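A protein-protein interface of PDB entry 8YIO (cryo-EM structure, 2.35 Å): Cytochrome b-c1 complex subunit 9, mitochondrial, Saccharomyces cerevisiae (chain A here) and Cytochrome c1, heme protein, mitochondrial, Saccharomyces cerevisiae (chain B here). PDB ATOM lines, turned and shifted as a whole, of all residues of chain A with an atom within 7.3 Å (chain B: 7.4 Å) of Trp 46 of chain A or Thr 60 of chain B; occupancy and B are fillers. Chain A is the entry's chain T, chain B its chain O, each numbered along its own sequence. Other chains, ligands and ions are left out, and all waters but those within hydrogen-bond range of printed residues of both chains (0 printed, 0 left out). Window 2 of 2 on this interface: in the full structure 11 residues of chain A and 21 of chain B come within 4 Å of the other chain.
Of the 11 printed residues of chain A, 4 touch a printed residue of chain B. Of the 21 printed residues of chain B, 9 touch a printed residue of chain A. Hydrophobic or aromatic side chains of chain B within 4 Å of the printed part of chain A: His 26. Among the printed residues, no Asp or Glu carboxylate lies within 4 Å of a Lys or Arg side-chain nitrogen of the other chain.
Phe 24 of chain B touches Lys 44 of chain A (O to O, 3.5 Å). O of Gly 56 of chain B touches CD1 of Trp 46 of chain A, 3.4 Å away. Trp 46 of chain A touches Val 57 of chain B. CZ3 of Trp 46 of chain A touches O of Ser 58 of chain B (3.2 Å). CZ2 of Trp 46 of chain A touches C of His 59 of chain B, 3.8 Å away. Thr 60 of chain B touches Trp 46 of chain A. Ala 27 of chain B touches Val 49 of chain A. Ile 53 of chain A touches Arg 30 of chain B.
The backbone NH (N) of His 26 of chain B sits at hydrogen-bond distance from the backbone carbonyl oxygen (O) of Lys 44 of chain A, at 3.1 Å.
The backbone NH of Thr 60 of chain B sits at hydrogen-bond distance from the side-chain carboxylate of Glu 63 of chain B, at 2.9 Å. NH1 of Arg 30 of chain B is in salt-bridge range of OE2 of Glu 63 of chain B (3.3 Å). The side-chain carboxylate (OD1) of Asp 203 of chain B lies within hydrogen-bond range of the backbone NH (N) of Phe 24 of chain B (3.2 Å). The backbone carbonyl oxygen of Ser 58 of chain B lies within hydrogen-bond range of the guanidinium group of Arg 30 of chain B (2.9 Å). OD2 of Asp 203 of chain B is in hydrogen-bond range of NE2 of His 26 of chain B, at 3.2 Å. The backbone carbonyl oxygen of Leu 54 of chain B sits at hydrogen-bond distance from the backbone NH of His 59 of chain B.
Of chain B, only Gly 56 (3.4 Å), Val 57 (3.6 Å), Ser 58 (3.2 Å), His 59 (3.8 Å) and Thr 60 (3.9 Å) come within 4 Å of Trp 46 of chain A. Thr 60 of chain B touches just one residue of chain A: Trp 46 (3.9 Å). Of the printed residues of chain A, His 26 of chain B touches Lys 44. Of the printed residues of chain A, Gly 56 of chain B touches Trp 46 (3.4 Å). Of the printed residues of chain A, Ser 58 of chain B touches Trp 46 (3.2 Å). Of the printed residues of chain A, Arg 30 of chain B touches Ile 53 (3.6 Å). Asn 66 of chain B touches none of the printed residues of chain A. The nearest residue of chain A that does not touch Thr 60 of chain B is Lys 50 of chain A (4.1 Å).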
ATOM      1  N   GLY A  43     -29.401   1.883 -10.047  1.00  0.00           N
ATOM      2  CA  GLY A  43     -29.884   2.356 -11.324  1.00  0.00           C
ATOM      3  C   GLY A  43     -30.563   3.707 -11.289  1.00  0.00           C
ATOM      4  O   GLY A  43     -30.921   4.228 -12.352  1.00  0.00           O
ATOM      5  N   LYS A  44     -30.753   4.293 -10.106  1.00  0.00           N
ATOM      6  CA  LYS A  44     -31.409   5.584  -9.972  1.00  0.00           C
ATOM      7  C   LYS A  44     -30.510   6.683  -9.433  1.00  0.00           C
ATOM      8  O   LYS A  44     -30.867   7.857  -9.563  1.00  0.00           O
ATOM      9  CB  LYS A  44     -32.638   5.474  -9.053  1.00  0.00           C
ATOM     10  CG  LYS A  44     -33.779   4.655  -9.623  1.00  0.00           C
ATOM     11  CD  LYS A  44     -35.087   4.967  -8.917  1.00  0.00           C
ATOM     12  CE  LYS A  44     -35.018   4.616  -7.444  1.00  0.00           C
ATOM     13  NZ  LYS A  44     -36.328   4.788  -6.767  1.00  0.00           N
ATOM     14  N   LEU A  45     -29.369   6.345  -8.841  1.00  0.00           N
ATOM     15  CA  LEU A  45     -28.484   7.338  -8.258  1.00  0.00           C
ATOM     16  C   LEU A  45     -27.696   8.059  -9.347  1.00  0.00           C
ATOM     17  O   LEU A  45     -27.667   7.647 -10.509  1.00  0.00           O
ATOM     18  CB  LEU A  45     -27.538   6.685  -7.255  1.00  0.00           C
ATOM     19  CG  LEU A  45     -28.201   5.807  -6.195  1.00  0.00           C
ATOM     20  CD1 LEU A  45     -27.157   5.038  -5.410  1.00  0.00           C
ATOM     21  CD2 LEU A  45     -29.062   6.643  -5.266  1.00  0.00           C
ATOM     22  N   TRP A  46     -27.049   9.161  -8.956  1.00  0.00           N
ATOM     23  CA  TRP A  46     -26.256   9.930  -9.907  1.00  0.00           C
ATOM     24  C   TRP A  46     -24.996   9.184 -10.328  1.00  0.00           C
ATOM     25  O   TRP A  46     -24.535   9.346 -11.464  1.00  0.00           O
ATOM     26  CB  TRP A  46     -25.905  11.303  -9.319  1.00  0.00           C
ATOM     27  CG  TRP A  46     -24.848  12.042 -10.089  1.00  0.00           C
ATOM     28  CD1 TRP A  46     -23.589  12.347  -9.667  1.00  0.00           C
ATOM     29  CD2 TRP A  46     -24.950  12.539 -11.430  1.00  0.00           C
ATOM     30  NE1 TRP A  46     -22.906  13.013 -10.651  1.00  0.00           N
ATOM     31  CE2 TRP A  46     -23.718  13.141 -11.745  1.00  0.00           C
ATOM     32  CE3 TRP A  46     -25.965  12.535 -12.393  1.00  0.00           C
ATOM     33  CZ2 TRP A  46     -23.475  13.737 -12.980  1.00  0.00           C
ATOM     34  CZ3 TRP A  46     -25.721  13.122 -13.615  1.00  0.00           C
ATOM     35  CH2 TRP A  46     -24.485  13.718 -13.898  1.00  0.00           C
ATOM     36  N   LYS A  47     -24.443   8.343  -9.450  1.00  0.00           N
ATOM     37  CA  LYS A  47     -23.258   7.576  -9.821  1.00  0.00           C
ATOM     38  C   LYS A  47     -23.586   6.484 -10.835  1.00  0.00           C
ATOM     39  O   LYS A  47     -22.723   6.112 -11.636  1.00  0.00           O
ATOM     40  CB  LYS A  47     -22.587   6.991  -8.573  1.00  0.00           C
ATOM     41  CG  LYS A  47     -23.310   5.823  -7.925  1.00  0.00           C
ATOM     42  CD  LYS A  47     -22.734   5.478  -6.568  1.00  0.00           C
ATOM     43  CE  LYS A  47     -23.461   4.286  -5.971  1.00  0.00           C
ATOM     44  NZ  LYS A  47     -23.516   3.145  -6.928  1.00  0.00           N
ATOM     45  N   ASP A  48     -24.821   5.979 -10.840  1.00  0.00           N
ATOM     46  CA  ASP A  48     -25.233   5.026 -11.860  1.00  0.00           C
ATOM     47  C   ASP A  48     -25.637   5.716 -13.152  1.00  0.00           C
ATOM     48  O   ASP A  48     -25.666   5.070 -14.203  1.00  0.00           O
ATOM     49  CB  ASP A  48     -26.392   4.165 -11.348  1.00  0.00           C
ATOM     50  CG  ASP A  48     -26.023   3.368 -10.112  1.00  0.00           C
ATOM     51  OD1 ASP A  48     -24.893   2.844 -10.056  1.00  0.00           O
ATOM     52  OD2 ASP A  48     -26.863   3.268  -9.194  1.00  0.00           O
ATOM     53  N   VAL A  49     -25.942   7.007 -13.091  1.00  0.00           N
ATOM     54  CA  VAL A  49     -26.251   7.792 -14.281  1.00  0.00           C
ATOM     55  C   VAL A  49     -24.977   8.273 -14.964  1.00  0.00           C
ATOM     56  O   VAL A  49     -24.847   8.156 -16.182  1.00  0.00           O
ATOM     57  CB  VAL A  49     -27.183   8.961 -13.891  1.00  0.00           C
ATOM     58  CG1 VAL A  49     -27.217  10.037 -14.963  1.00  0.00           C
ATOM     59  CG2 VAL A  49     -28.587   8.448 -13.619  1.00  0.00           C
ATOM     60  N   LYS A  50     -24.003   8.756 -14.179  1.00  0.00           N
ATOM     61  CA  LYS A  50     -22.754   9.288 -14.724  1.00  0.00           C
ATOM     62  C   LYS A  50     -21.935   8.212 -15.438  1.00  0.00           C
ATOM     63  O   LYS A  50     -21.209   8.512 -16.394  1.00  0.00           O
ATOM     64  CB  LYS A  50     -21.947   9.935 -13.591  1.00  0.00           C
ATOM     65  CG  LYS A  50     -20.591  10.504 -13.982  1.00  0.00           C
ATOM     66  CD  LYS A  50     -19.739  10.851 -12.777  1.00  0.00           C
ATOM     67  CE  LYS A  50     -19.165  12.251 -12.908  1.00  0.00           C
ATOM     68  NZ  LYS A  50     -18.426  12.678 -11.691  1.00  0.00           N
ATOM     69  N   ALA A  51     -22.096   6.948 -15.044  1.00  0.00           N
ATOM     70  CA  ALA A  51     -21.362   5.843 -15.648  1.00  0.00           C
ATOM     71  C   ALA A  51     -21.784   5.529 -17.081  1.00  0.00           C
ATOM     72  O   ALA A  51     -21.096   4.745 -17.743  1.00  0.00           O
ATOM     73  CB  ALA A  51     -21.510   4.586 -14.788  1.00  0.00           C
ATOM     74  N   ARG A  52     -22.887   6.100 -17.585  1.00  0.00           N
ATOM     75  CA  ARG A  52     -23.218   5.923 -18.994  1.00  0.00           C
ATOM     76  C   ARG A  52     -23.728   7.192 -19.674  1.00  0.00           C
ATOM     77  O   ARG A  52     -24.155   7.121 -20.833  1.00  0.00           O
ATOM     78  CB  ARG A  52     -24.227   4.784 -19.181  1.00  0.00           C
ATOM     79  CG  ARG A  52     -25.595   5.012 -18.580  1.00  0.00           C
ATOM     80  CD  ARG A  52     -26.448   3.770 -18.780  1.00  0.00           C
ATOM     81  NE  ARG A  52     -27.809   3.941 -18.288  1.00  0.00           N
ATOM     82  CZ  ARG A  52     -28.189   3.679 -17.042  1.00  0.00           C
ATOM     83  NH1 ARG A  52     -27.310   3.228 -16.158  1.00  0.00           N
ATOM     84  NH2 ARG A  52     -29.451   3.863 -16.683  1.00  0.00           N
ATOM     85  N   ILE A  53     -23.702   8.339 -19.003  1.00  0.00           N
ATOM     86  CA  ILE A  53     -23.803   9.643 -19.653  1.00  0.00           C
ATOM     87  C   ILE A  53     -22.400  10.139 -20.032  1.00  0.00           C
ATOM     88  O   ILE A  53     -22.241  11.095 -20.794  1.00  0.00           O
ATOM     89  CB  ILE A  53     -24.596  10.626 -18.757  1.00  0.00           C
ATOM     90  CG1 ILE A  53     -25.992  10.060 -18.492  1.00  0.00           C
ATOM     91  CG2 ILE A  53     -24.864  12.003 -19.372  1.00  0.00           C
ATOM     92  CD1 ILE A  53     -26.823   9.820 -19.749  1.00  0.00           C
ATOM     93  N   PHE B  24     -35.049   9.699  -5.513  1.00  0.00           N
ATOM     94  CA  PHE B  24     -35.427  10.246  -6.807  1.00  0.00           C
ATOM     95  C   PHE B  24     -34.786   9.439  -7.931  1.00  0.00           C
ATOM     96  O   PHE B  24     -33.761   8.780  -7.748  1.00  0.00           O
ATOM     97  CB  PHE B  24     -34.993  11.708  -6.927  1.00  0.00           C
ATOM     98  CG  PHE B  24     -35.905  12.684  -6.240  1.00  0.00           C
ATOM     99  CD1 PHE B  24     -37.274  12.635  -6.434  1.00  0.00           C
ATOM    100  CD2 PHE B  24     -35.384  13.666  -5.415  1.00  0.00           C
ATOM    101  CE1 PHE B  24     -38.109  13.540  -5.803  1.00  0.00           C
ATOM    102  CE2 PHE B  24     -36.212  14.573  -4.784  1.00  0.00           C
ATOM    103  CZ  PHE B  24     -37.578  14.507  -4.977  1.00  0.00           C
ATOM    104  N   ASP B  25     -35.406   9.489  -9.104  1.00  0.00           N
ATOM    105  CA  ASP B  25     -34.798   8.989 -10.332  1.00  0.00           C
ATOM    106  C   ASP B  25     -34.008  10.139 -10.946  1.00  0.00           C
ATOM    107  O   ASP B  25     -34.592  11.096 -11.462  1.00  0.00           O
ATOM    108  CB  ASP B  25     -35.865   8.463 -11.288  1.00  0.00           C
ATOM    109  CG  ASP B  25     -35.280   7.803 -12.525  1.00  0.00           C
ATOM    110  OD1 ASP B  25     -34.074   7.488 -12.538  1.00  0.00           O
ATOM    111  OD2 ASP B  25     -36.036   7.593 -13.492  1.00  0.00           O
ATOM    112  N   HIS B  26     -32.680  10.047 -10.894  1.00  0.00           N
ATOM    113  CA  HIS B  26     -31.837  11.177 -11.262  1.00  0.00           C
ATOM    114  C   HIS B  26     -31.675  11.343 -12.766  1.00  0.00           C
ATOM    115  O   HIS B  26     -31.279  12.422 -13.214  1.00  0.00           O
ATOM    116  CB  HIS B  26     -30.470  11.043 -10.594  1.00  0.00           C
ATOM    117  CG  HIS B  26     -30.482  11.383  -9.137  1.00  0.00           C
ATOM    118  ND1 HIS B  26     -29.956  12.555  -8.641  1.00  0.00           N
ATOM    119  CD2 HIS B  26     -30.973  10.712  -8.070  1.00  0.00           C
ATOM    120  CE1 HIS B  26     -30.113  12.588  -7.332  1.00  0.00           C
ATOM    121  NE2 HIS B  26     -30.729  11.481  -6.960  1.00  0.00           N
ATOM    122  N   ALA B  27     -31.974  10.312 -13.557  1.00  0.00           N
ATOM    123  CA  ALA B  27     -32.023  10.488 -15.002  1.00  0.00           C
ATOM    124  C   ALA B  27     -33.279  11.231 -15.433  1.00  0.00           C
ATOM    125  O   ALA B  27     -33.251  11.963 -16.428  1.00  0.00           O
ATOM    126  CB  ALA B  27     -31.947   9.132 -15.703  1.00  0.00           C
ATOM    127  N   ARG B  30     -32.579  14.941 -14.801  1.00  0.00           N
ATOM    128  CA  ARG B  30     -31.719  15.546 -15.814  1.00  0.00           C
ATOM    129  C   ARG B  30     -32.494  15.867 -17.088  1.00  0.00           C
ATOM    130  O   ARG B  30     -32.295  16.929 -17.687  1.00  0.00           O
ATOM    131  CB  ARG B  30     -30.542  14.617 -16.113  1.00  0.00           C
ATOM    132  CG  ARG B  30     -29.580  15.128 -17.167  1.00  0.00           C
ATOM    133  CD  ARG B  30     -28.481  14.120 -17.445  1.00  0.00           C
ATOM    134  NE  ARG B  30     -27.663  14.502 -18.591  1.00  0.00           N
ATOM    135  CZ  ARG B  30     -26.503  15.144 -18.506  1.00  0.00           C
ATOM    136  NH1 ARG B  30     -25.833  15.447 -19.604  1.00  0.00           N
ATOM    137  NH2 ARG B  30     -26.014  15.484 -17.325  1.00  0.00           N
ATOM    138  N   LEU B  54     -26.916  21.940  -8.508  1.00  0.00           N
ATOM    139  CA  LEU B  54     -27.091  20.964  -9.576  1.00  0.00           C
ATOM    140  C   LEU B  54     -25.904  20.023  -9.736  1.00  0.00           C
ATOM    141  O   LEU B  54     -26.044  18.996 -10.405  1.00  0.00           O
ATOM    142  CB  LEU B  54     -27.339  21.670 -10.911  1.00  0.00           C
ATOM    143  CG  LEU B  54     -28.600  22.505 -11.123  1.00  0.00           C
ATOM    144  CD1 LEU B  54     -28.500  23.242 -12.440  1.00  0.00           C
ATOM    145  CD2 LEU B  54     -29.835  21.639 -11.105  1.00  0.00           C
ATOM    146  N   VAL B  55     -24.751  20.343  -9.156  1.00  0.00           N
ATOM    147  CA  VAL B  55     -23.548  19.534  -9.330  1.00  0.00           C
ATOM    148  C   VAL B  55     -23.655  18.280  -8.474  1.00  0.00           C
ATOM    149  O   VAL B  55     -23.906  18.356  -7.266  1.00  0.00           O
ATOM    150  CB  VAL B  55     -22.291  20.344  -8.971  1.00  0.00           C
ATOM    151  CG1 VAL B  55     -21.041  19.510  -9.172  1.00  0.00           C
ATOM    152  CG2 VAL B  55     -22.224  21.614  -9.797  1.00  0.00           C
ATOM    153  N   GLY B  56     -23.459  17.121  -9.098  1.00  0.00           N
ATOM    154  CA  GLY B  56     -23.573  15.855  -8.410  1.00  0.00           C
ATOM    155  C   GLY B  56     -24.984  15.350  -8.234  1.00  0.00           C
ATOM    156  O   GLY B  56     -25.190  14.386  -7.490  1.00  0.00           O
ATOM    157  N   VAL B  57     -25.963  15.976  -8.883  1.00  0.00           N
ATOM    158  CA  VAL B  57     -27.359  15.568  -8.797  1.00  0.00           C
ATOM    159  C   VAL B  57     -27.852  15.283 -10.209  1.00  0.00           C
ATOM    160  O   VAL B  57     -28.447  14.233 -10.473  1.00  0.00           O
ATOM    161  CB  VAL B  57     -28.219  16.641  -8.097  1.00  0.00           C
ATOM    162  CG1 VAL B  57     -29.700  16.326  -8.224  1.00  0.00           C
ATOM    163  CG2 VAL B  57     -27.838  16.771  -6.632  1.00  0.00           C
ATOM    164  N   SER B  58     -27.592  16.208 -11.130  1.00  0.00           N
ATOM    165  CA  SER B  58     -28.003  16.048 -12.518  1.00  0.00           C
ATOM    166  C   SER B  58     -26.923  16.371 -13.542  1.00  0.00           C
ATOM    167  O   SER B  58     -27.031  15.898 -14.680  1.00  0.00           O
ATOM    168  CB  SER B  58     -29.236  16.914 -12.813  1.00  0.00           C
ATOM    169  OG  SER B  58     -29.034  18.250 -12.395  1.00  0.00           O
ATOM    170  N   HIS B  59     -25.894  17.143 -13.195  1.00  0.00           N
ATOM    171  CA  HIS B  59     -24.857  17.530 -14.141  1.00  0.00           C
ATOM    172  C   HIS B  59     -23.496  17.460 -13.463  1.00  0.00           C
ATOM    173  O   HIS B  59     -23.394  17.450 -12.235  1.00  0.00           O
ATOM    174  CB  HIS B  59     -25.090  18.945 -14.692  1.00  0.00           C
ATOM    175  CG  HIS B  59     -26.360  19.100 -15.471  1.00  0.00           C
ATOM    176  ND1 HIS B  59     -27.588  19.267 -14.870  1.00  0.00           N
ATOM    177  CD2 HIS B  59     -26.588  19.128 -16.804  1.00  0.00           C
ATOM    178  CE1 HIS B  59     -28.520  19.381 -15.799  1.00  0.00           C
ATOM    179  NE2 HIS B  59     -27.939  19.299 -16.982  1.00  0.00           N
ATOM    180  N   THR B  60     -22.442  17.417 -14.279  1.00  0.00           N
ATOM    181  CA  THR B  60     -21.080  17.459 -13.762  1.00  0.00           C
ATOM    182  C   THR B  60     -20.664  18.906 -13.499  1.00  0.00           C
ATOM    183  O   THR B  60     -21.390  19.851 -13.805  1.00  0.00           O
ATOM    184  CB  THR B  60     -20.107  16.777 -14.726  1.00  0.00           C
ATOM    185  OG1 THR B  60     -19.941  17.580 -15.900  1.00  0.00           O
ATOM    186  CG2 THR B  60     -20.615  15.408 -15.124  1.00  0.00           C
ATOM    187  N   ASN B  61     -19.465  19.079 -12.937  1.00  0.00           N
ATOM    188  CA  ASN B  61     -19.039  20.394 -12.460  1.00  0.00           C
ATOM    189  C   ASN B  61     -18.727  21.348 -13.608  1.00  0.00           C
ATOM    190  O   ASN B  61     -19.019  22.545 -13.518  1.00  0.00           O
ATOM    191  CB  ASN B  61     -17.811  20.241 -11.565  1.00  0.00           C
ATOM    192  CG  ASN B  61     -17.302  21.568 -11.039  1.00  0.00           C
ATOM    193  OD1 ASN B  61     -16.343  22.130 -11.561  1.00  0.00           O
ATOM    194  ND2 ASN B  61     -17.942  22.070  -9.996  1.00  0.00           N
ATOM    195  N   GLU B  62     -18.139  20.849 -14.694  1.00  0.00           N
ATOM    196  CA  GLU B  62     -17.856  21.722 -15.824  1.00  0.00           C
ATOM    197  C   GLU B  62     -19.061  21.915 -16.735  1.00  0.00           C
ATOM    198  O   GLU B  62     -19.056  22.837 -17.555  1.00  0.00           O
ATOM    199  CB  GLU B  62     -16.665  21.193 -16.631  1.00  0.00           C
ATOM    200  CG  GLU B  62     -16.897  19.874 -17.343  1.00  0.00           C
ATOM    201  CD  GLU B  62     -16.528  18.667 -16.495  1.00  0.00           C
ATOM    202  OE1 GLU B  62     -16.363  18.816 -15.266  1.00  0.00           O
ATOM    203  OE2 GLU B  62     -16.400  17.562 -17.064  1.00  0.00           O
ATOM    204  N   GLU B  63     -20.092  21.079 -16.607  1.00  0.00           N
ATOM    205  CA  GLU B  63     -21.327  21.320 -17.346  1.00  0.00           C
ATOM    206  C   GLU B  63     -22.093  22.506 -16.773  1.00  0.00           C
ATOM    207  O   GLU B  63     -22.667  23.298 -17.527  1.00  0.00           O
ATOM    208  CB  GLU B  63     -22.200  20.068 -17.339  1.00  0.00           C
ATOM    209  CG  GLU B  63     -21.819  19.043 -18.382  1.00  0.00           C
ATOM    210  CD  GLU B  63     -22.647  17.779 -18.282  1.00  0.00           C
ATOM    211  OE1 GLU B  63     -22.909  17.325 -17.150  1.00  0.00           O
ATOM    212  OE2 GLU B  63     -23.036  17.238 -19.336  1.00  0.00           O
ATOM    213  N   VAL B  64     -22.110  22.646 -15.446  1.00  0.00           N
ATOM    214  CA  VAL B  64     -22.844  23.744 -14.825  1.00  0.00           C
ATOM    215  C   VAL B  64     -22.096  25.065 -14.994  1.00  0.00           C
ATOM    216  O   VAL B  64     -22.723  26.127 -15.089  1.00  0.00           O
ATOM    217  CB  VAL B  64     -23.128  23.424 -13.344  1.00  0.00           C
ATOM    218  CG1 VAL B  64     -24.075  24.434 -12.727  1.00  0.00           C
ATOM    219  CG2 VAL B  64     -23.738  22.058 -13.216  1.00  0.00           C
ATOM    220  N   ARG B  65     -20.760  25.020 -15.054  1.00  0.00           N
ATOM    221  CA  ARG B  65     -19.974  26.229 -15.289  1.00  0.00           C
ATOM    222  C   ARG B  65     -20.261  26.824 -16.663  1.00  0.00           C
ATOM    223  O   ARG B  65     -20.309  28.048 -16.818  1.00  0.00           O
ATOM    224  CB  ARG B  65     -18.484  25.927 -15.154  1.00  0.00           C
ATOM    225  CG  ARG B  65     -17.981  25.783 -13.735  1.00  0.00           C
ATOM    226  CD  ARG B  65     -16.473  25.613 -13.718  1.00  0.00           C
ATOM    227  NE  ARG B  65     -15.998  25.055 -12.457  1.00  0.00           N
ATOM    228  CZ  ARG B  65     -15.593  25.781 -11.422  1.00  0.00           C
ATOM    229  NH1 ARG B  65     -15.600  27.104 -11.493  1.00  0.00           N
ATOM    230  NH2 ARG B  65     -15.181  25.184 -10.313  1.00  0.00           N
ATOM    231  N   ASN B  66     -20.474  25.972 -17.667  1.00  0.00           N
ATOM    232  CA  ASN B  66     -20.792  26.467 -19.002  1.00  0.00           C
ATOM    233  C   ASN B  66     -22.227  26.968 -19.094  1.00  0.00           C
ATOM    234  O   ASN B  66     -22.516  27.854 -19.904  1.00  0.00           O
ATOM    235  CB  ASN B  66     -20.494  25.398 -20.051  1.00  0.00           C
ATOM    236  CG  ASN B  66     -19.011  25.192 -20.265  1.00  0.00           C
ATOM    237  OD1 ASN B  66     -18.226  26.135 -20.206  1.00  0.00           O
ATOM    238  ND2 ASN B  66     -18.618  23.950 -20.509  1.00  0.00           N
ATOM    239  N   MET B  67     -23.133  26.411 -18.287  1.00  0.00           N
ATOM    240  CA  MET B  67     -24.521  26.858 -18.309  1.00  0.00           C
ATOM    241  C   MET B  67     -24.668  28.234 -17.670  1.00  0.00           C
ATOM    242  O   MET B  67     -25.413  29.081 -18.175  1.00  0.00           O
ATOM    243  CB  MET B  67     -25.417  25.841 -17.600  1.00  0.00           C
ATOM    244  CG  MET B  67     -25.639  24.550 -18.373  1.00  0.00           C
ATOM    245  SD  MET B  67     -26.937  23.496 -17.695  1.00  0.00           S
ATOM    246  CE  MET B  67     -26.365  23.259 -16.021  1.00  0.00           C
ATOM    247  N   LEU B  90     -20.905  29.803 -10.108  1.00  0.00           N
ATOM    248  CA  LEU B  90     -21.686  28.808  -9.378  1.00  0.00           C
ATOM    249  C   LEU B  90     -22.354  29.372  -8.130  1.00  0.00           C
ATOM    250  O   LEU B  90     -23.285  28.752  -7.611  1.00  0.00           O
ATOM    251  CB  LEU B  90     -20.808  27.615  -8.996  1.00  0.00           C
ATOM    252  CG  LEU B  90     -20.288  26.703 -10.110  1.00  0.00           C
ATOM    253  CD1 LEU B  90     -19.870  25.363  -9.542  1.00  0.00           C
ATOM    254  CD2 LEU B  90     -21.308  26.511 -11.215  1.00  0.00           C
ATOM    255  N   ASP B 203     -33.491  12.743  -0.513  1.00  0.00           N
ATOM    256  CA  ASP B 203     -32.770  11.474  -0.473  1.00  0.00           C
ATOM    257  C   ASP B 203     -31.997  11.298   0.827  1.00  0.00           C
ATOM    258  O   ASP B 203     -31.841  10.173   1.305  1.00  0.00           O
ATOM    259  CB  ASP B 203     -31.823  11.364  -1.668  1.00  0.00           C
ATOM    260  CG  ASP B 203     -32.558  11.194  -2.979  1.00  0.00           C
ATOM    261  OD1 ASP B 203     -33.803  11.240  -2.975  1.00  0.00           O
ATOM    262  OD2 ASP B 203     -31.895  11.009  -4.017  1.00  0.00           O
